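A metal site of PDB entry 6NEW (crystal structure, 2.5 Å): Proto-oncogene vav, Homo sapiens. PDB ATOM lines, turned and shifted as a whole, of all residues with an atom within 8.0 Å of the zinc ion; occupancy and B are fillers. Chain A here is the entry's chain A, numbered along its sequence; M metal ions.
Within 4 Å of the zinc ion: His 362, Cys 392, Cys 395 and Cys 410. Along chain A the residues within 4 Å of the zinc ion span positions 362 to 410. The nearest printed residue that does not touch the zinc ion is Arg 394 (4.4 Å).
A ring nitrogen (NE2) of His 362 lies within hydrogen-bond range of the backbone carbonyl oxygen (O) of Pro 408 (2.9 Å). SG of Cys 392 lies close to N of Arg 394 (3.7 Å). NH1 of Arg 394 sits at hydrogen-bond distance from O of His 362 (3.4 Å). The side-chain sulfur (SG) of Cys 392 sits close to the backbone NH (N) of Asp 363 (3.4 Å). The backbone carbonyl oxygen (O) of Gly 361 sits close to the side-chain sulfur (SG) of Cys 410. SG of Cys 395 sits close to N of Ala 397 (3.4 Å). The backbone NH (N) of Cys 392 sits at hydrogen-bond distance from the backbone carbonyl oxygen (O) of Ala 397 (2.9 Å). N of Cys 410 sits at hydrogen-bond distance from O of Asn 360.
The zinc ion is bound by a ring nitrogen (ND1) of His 362. The zinc ion is bound by SG of Cys 392, 2.3 Å away. The zinc ion is bound by SG of Cys 395, at 2.3 Å. SG of Cys 410 is bound to the zinc ion (2.3 Å).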
ATOM      1  N   ALA A 357      -9.576  -3.426  23.073  1.00  0.00           N
ATOM      2  CA  ALA A 357      -9.175  -2.024  22.905  1.00  0.00           C
ATOM      3  C   ALA A 357     -10.211  -1.301  22.065  1.00  0.00           C
ATOM      4  O   ALA A 357     -10.453  -0.107  22.254  1.00  0.00           O
ATOM      5  CB  ALA A 357      -7.811  -1.954  22.236  1.00  0.00           C
ATOM      6  N   ALA A 359     -13.452  -2.617  21.839  1.00  0.00           N
ATOM      7  CA  ALA A 359     -14.748  -3.118  22.262  1.00  0.00           C
ATOM      8  C   ALA A 359     -15.747  -1.964  22.405  1.00  0.00           C
ATOM      9  O   ALA A 359     -15.375  -0.845  22.786  1.00  0.00           O
ATOM     10  CB  ALA A 359     -14.629  -3.853  23.596  1.00  0.00           C
ATOM     11  N   ASN A 360     -17.017  -2.236  22.034  1.00  0.00           N
ATOM     12  CA  ASN A 360     -18.170  -1.335  22.150  1.00  0.00           C
ATOM     13  C   ASN A 360     -17.928   0.097  21.637  1.00  0.00           C
ATOM     14  O   ASN A 360     -18.261   1.056  22.326  1.00  0.00           O
ATOM     15  CB  ASN A 360     -18.667  -1.325  23.613  1.00  0.00           C
ATOM     16  CG  ASN A 360     -18.776  -2.702  24.253  1.00  0.00           C
ATOM     17  OD1 ASN A 360     -18.158  -2.974  25.290  1.00  0.00           O
ATOM     18  ND2 ASN A 360     -19.521  -3.604  23.635  1.00  0.00           N
ATOM     19  N   GLY A 361     -17.336   0.212  20.442  1.00  0.00           N
ATOM     20  CA  GLY A 361     -17.089   1.512  19.812  1.00  0.00           C
ATOM     21  C   GLY A 361     -15.869   2.306  20.233  1.00  0.00           C
ATOM     22  O   GLY A 361     -15.601   3.376  19.679  1.00  0.00           O
ATOM     23  N   HIS A 362     -15.129   1.839  21.223  1.00  0.00           N
ATOM     24  CA  HIS A 362     -13.972   2.596  21.685  1.00  0.00           C
ATOM     25  C   HIS A 362     -12.726   2.378  20.811  1.00  0.00           C
ATOM     26  O   HIS A 362     -12.732   1.594  19.863  1.00  0.00           O
ATOM     27  CB  HIS A 362     -13.639   2.200  23.133  1.00  0.00           C
ATOM     28  CG  HIS A 362     -14.750   2.443  24.120  1.00  0.00           C
ATOM     29  ND1 HIS A 362     -15.098   3.729  24.519  1.00  0.00           N
ATOM     30  CD2 HIS A 362     -15.489   1.553  24.817  1.00  0.00           C
ATOM     31  CE1 HIS A 362     -16.046   3.573  25.414  1.00  0.00           C
ATOM     32  NE2 HIS A 362     -16.325   2.286  25.622  1.00  0.00           N
ATOM     33  N   ASP A 363     -11.676   3.133  21.152  1.00  0.00           N
ATOM     34  CA  ASP A 363     -10.332   3.033  20.612  1.00  0.00           C
ATOM     35  C   ASP A 363      -9.401   3.385  21.764  1.00  0.00           C
ATOM     36  O   ASP A 363      -8.963   4.533  21.900  1.00  0.00           O
ATOM     37  CB  ASP A 363     -10.094   3.890  19.351  1.00  0.00           C
ATOM     38  CG  ASP A 363      -8.729   3.650  18.701  1.00  0.00           C
ATOM     39  OD1 ASP A 363      -8.126   2.558  18.954  1.00  0.00           O
ATOM     40  OD2 ASP A 363      -8.259   4.535  17.963  1.00  0.00           O
ATOM     41  N   PHE A 364      -9.201   2.398  22.642  1.00  0.00           N
ATOM     42  CA  PHE A 364      -8.371   2.572  23.819  1.00  0.00           C
ATOM     43  C   PHE A 364      -6.915   2.532  23.459  1.00  0.00           C
ATOM     44  O   PHE A 364      -6.454   1.585  22.831  1.00  0.00           O
ATOM     45  CB  PHE A 364      -8.690   1.520  24.909  1.00  0.00           C
ATOM     46  CG  PHE A 364      -9.992   1.769  25.649  1.00  0.00           C
ATOM     47  CD1 PHE A 364     -10.107   2.826  26.550  1.00  0.00           C
ATOM     48  CD2 PHE A 364     -11.073   0.910  25.488  1.00  0.00           C
ATOM     49  CE1 PHE A 364     -11.286   3.019  27.273  1.00  0.00           C
ATOM     50  CE2 PHE A 364     -12.249   1.094  26.223  1.00  0.00           C
ATOM     51  CZ  PHE A 364     -12.352   2.163  27.084  1.00  0.00           C
ATOM     52  N   ARG A 391      -6.840   5.431  27.468  1.00  0.00           N
ATOM     53  CA  ARG A 391      -7.839   6.432  27.185  1.00  0.00           C
ATOM     54  C   ARG A 391      -8.397   6.204  25.807  1.00  0.00           C
ATOM     55  O   ARG A 391      -7.661   5.903  24.861  1.00  0.00           O
ATOM     56  CB  ARG A 391      -7.295   7.856  27.349  1.00  0.00           C
ATOM     57  CG  ARG A 391      -8.391   8.896  27.565  1.00  0.00           C
ATOM     58  CD  ARG A 391      -7.909  10.273  27.189  1.00  0.00           C
ATOM     59  NE  ARG A 391      -7.451  10.314  25.791  1.00  0.00           N
ATOM     60  CZ  ARG A 391      -7.164  11.423  25.135  1.00  0.00           C
ATOM     61  NH1 ARG A 391      -7.270  12.610  25.719  1.00  0.00           N
ATOM     62  NH2 ARG A 391      -6.752  11.353  23.862  1.00  0.00           N
ATOM     63  N   CYS A 392      -9.721   6.313  25.696  1.00  0.00           N
ATOM     64  CA  CYS A 392     -10.394   6.231  24.400  1.00  0.00           C
ATOM     65  C   CYS A 392     -10.317   7.648  23.877  1.00  0.00           C
ATOM     66  O   CYS A 392     -10.815   8.556  24.539  1.00  0.00           O
ATOM     67  CB  CYS A 392     -11.833   5.751  24.538  1.00  0.00           C
ATOM     68  SG  CYS A 392     -12.777   5.820  22.995  1.00  0.00           S
ATOM     69  N   HIS A 393      -9.635   7.885  22.744  1.00  0.00           N
ATOM     70  CA  HIS A 393      -9.471   9.260  22.251  1.00  0.00           C
ATOM     71  C   HIS A 393     -10.815   9.893  21.781  1.00  0.00           C
ATOM     72  O   HIS A 393     -10.958  11.113  21.842  1.00  0.00           O
ATOM     73  CB  HIS A 393      -8.366   9.345  21.168  1.00  0.00           C
ATOM     74  CG  HIS A 393      -8.799   8.880  19.819  1.00  0.00           C
ATOM     75  ND1 HIS A 393      -9.239   7.594  19.599  1.00  0.00           N
ATOM     76  CD2 HIS A 393      -8.860   9.572  18.655  1.00  0.00           C
ATOM     77  CE1 HIS A 393      -9.561   7.536  18.321  1.00  0.00           C
ATOM     78  NE2 HIS A 393      -9.336   8.698  17.701  1.00  0.00           N
ATOM     79  N   ARG A 394     -11.808   9.052  21.399  1.00  0.00           N
ATOM     80  CA  ARG A 394     -13.141   9.472  20.965  1.00  0.00           C
ATOM     81  C   ARG A 394     -14.037  10.004  22.083  1.00  0.00           C
ATOM     82  O   ARG A 394     -14.568  11.112  21.961  1.00  0.00           O
ATOM     83  CB  ARG A 394     -13.884   8.321  20.278  1.00  0.00           C
ATOM     84  CG  ARG A 394     -13.323   7.943  18.948  1.00  0.00           C
ATOM     85  CD  ARG A 394     -13.616   6.491  18.714  1.00  0.00           C
ATOM     86  NE  ARG A 394     -12.846   5.987  17.583  1.00  0.00           N
ATOM     87  CZ  ARG A 394     -12.976   4.762  17.088  1.00  0.00           C
ATOM     88  NH1 ARG A 394     -13.829   3.912  17.625  1.00  0.00           N
ATOM     89  NH2 ARG A 394     -12.250   4.400  16.036  1.00  0.00           N
ATOM     90  N   CYS A 395     -14.252   9.203  23.148  1.00  0.00           N
ATOM     91  CA  CYS A 395     -15.148   9.588  24.246  1.00  0.00           C
ATOM     92  C   CYS A 395     -14.423  10.116  25.468  1.00  0.00           C
ATOM     93  O   CYS A 395     -15.073  10.596  26.393  1.00  0.00           O
ATOM     94  CB  CYS A 395     -16.085   8.440  24.598  1.00  0.00           C
ATOM     95  SG  CYS A 395     -15.274   7.092  25.509  1.00  0.00           S
ATOM     96  N   ARG A 396     -13.087   9.945  25.504  1.00  0.00           N
ATOM     97  CA  ARG A 396     -12.169  10.342  26.576  1.00  0.00           C
ATOM     98  C   ARG A 396     -12.385   9.517  27.856  1.00  0.00           C
ATOM     99  O   ARG A 396     -11.894   9.916  28.919  1.00  0.00           O
ATOM    100  CB  ARG A 396     -12.199  11.883  26.814  1.00  0.00           C
ATOM    101  CG  ARG A 396     -11.882  12.669  25.536  1.00  0.00           C
ATOM    102  CD  ARG A 396     -11.963  14.155  25.710  1.00  0.00           C
ATOM    103  NE  ARG A 396     -10.617  14.712  25.890  1.00  0.00           N
ATOM    104  CZ  ARG A 396     -10.130  15.115  27.073  1.00  0.00           C
ATOM    105  NH1 ARG A 396      -8.890  15.596  27.150  1.00  0.00           N
ATOM    106  NH2 ARG A 396     -10.872  15.046  28.165  1.00  0.00           N
ATOM    107  N   ALA A 397     -13.020   8.336  27.732  1.00  0.00           N
ATOM    108  CA  ALA A 397     -13.148   7.423  28.873  1.00  0.00           C
ATOM    109  C   ALA A 397     -11.760   6.853  29.218  1.00  0.00           C
ATOM    110  O   ALA A 397     -10.990   6.480  28.328  1.00  0.00           O
ATOM    111  CB  ALA A 397     -14.103   6.290  28.561  1.00  0.00           C
ATOM    112  N   SER A 398     -11.432   6.899  30.494  1.00  0.00           N
ATOM    113  CA  SER A 398     -10.202   6.417  31.075  1.00  0.00           C
ATOM    114  C   SER A 398     -10.503   5.046  31.683  1.00  0.00           C
ATOM    115  O   SER A 398     -11.612   4.849  32.155  1.00  0.00           O
ATOM    116  CB  SER A 398      -9.746   7.398  32.149  1.00  0.00           C
ATOM    117  OG  SER A 398     -10.741   7.495  33.162  1.00  0.00           O
ATOM    118  N   VAL A 407     -16.114  -1.063  30.097  1.00  0.00           N
ATOM    119  CA  VAL A 407     -16.425   0.367  30.057  1.00  0.00           C
ATOM    120  C   VAL A 407     -17.741   0.539  29.256  1.00  0.00           C
ATOM    121  O   VAL A 407     -17.887  -0.102  28.222  1.00  0.00           O
ATOM    122  CB  VAL A 407     -15.256   1.210  29.470  1.00  0.00           C
ATOM    123  CG1 VAL A 407     -15.607   2.704  29.352  1.00  0.00           C
ATOM    124  CG2 VAL A 407     -13.986   1.037  30.289  1.00  0.00           C
ATOM    125  N   PRO A 408     -18.719   1.352  29.742  1.00  0.00           N
ATOM    126  CA  PRO A 408     -19.962   1.540  28.963  1.00  0.00           C
ATOM    127  C   PRO A 408     -19.692   1.990  27.508  1.00  0.00           C
ATOM    128  O   PRO A 408     -18.639   2.608  27.272  1.00  0.00           O
ATOM    129  CB  PRO A 408     -20.716   2.623  29.751  1.00  0.00           C
ATOM    130  CG  PRO A 408     -20.170   2.505  31.133  1.00  0.00           C
ATOM    131  CD  PRO A 408     -18.731   2.175  30.965  1.00  0.00           C
ATOM    132  N   PRO A 409     -20.607   1.682  26.538  1.00  0.00           N
ATOM    133  CA  PRO A 409     -20.362   2.011  25.123  1.00  0.00           C
ATOM    134  C   PRO A 409     -19.915   3.430  24.824  1.00  0.00           C
ATOM    135  O   PRO A 409     -20.225   4.372  25.549  1.00  0.00           O
ATOM    136  CB  PRO A 409     -21.695   1.689  24.452  1.00  0.00           C
ATOM    137  CG  PRO A 409     -22.228   0.591  25.252  1.00  0.00           C
ATOM    138  CD  PRO A 409     -21.870   0.921  26.679  1.00  0.00           C
ATOM    139  N   CYS A 410     -19.145   3.560  23.743  1.00  0.00           N
ATOM    140  CA  CYS A 410     -18.569   4.812  23.280  1.00  0.00           C
ATOM    141  C   CYS A 410     -19.638   5.792  22.800  1.00  0.00           C
ATOM    142  O   CYS A 410     -20.439   5.461  21.930  1.00  0.00           O
ATOM    143  CB  CYS A 410     -17.532   4.532  22.193  1.00  0.00           C
ATOM    144  SG  CYS A 410     -16.381   5.893  21.904  1.00  0.00           S
ATOM    145  N   GLY A 411     -19.605   6.961  23.411  1.00  0.00           N
ATOM    146  CA  GLY A 411     -20.476   8.069  23.141  1.00  0.00           C
ATOM    147  C   GLY A 411     -21.917   7.892  23.524  1.00  0.00           C
ATOM    148  O   GLY A 411     -22.788   8.188  22.742  1.00  0.00           O
ATOM    149  N   ARG A 412     -22.184   7.454  24.746  1.00  0.00           N
ATOM    150  CA  ARG A 412     -23.573   7.266  25.108  1.00  0.00           C
ATOM    151  C   ARG A 412     -24.059   7.909  26.386  1.00  0.00           C
ATOM    152  O   ARG A 412     -23.316   8.598  27.097  1.00  0.00           O
ATOM    153  CB  ARG A 412     -23.908   5.793  25.156  1.00  0.00           C
ATOM    154  CG  ARG A 412     -24.772   5.356  23.997  1.00  0.00           C
ATOM    155  CD  ARG A 412     -24.452   3.940  23.580  1.00  0.00           C
ATOM    156  NE  ARG A 412     -24.316   3.833  22.135  1.00  0.00           N
ATOM    157  CZ  ARG A 412     -24.585   2.735  21.452  1.00  0.00           C
ATOM    158  NH1 ARG A 412     -25.004   1.646  22.071  1.00  0.00           N
ATOM    159  NH2 ARG A 412     -24.436   2.734  20.137  1.00  0.00           N
HETATM  160 ZN    ZN M   1     -14.914   5.682  23.699  1.00  0.00          ZN
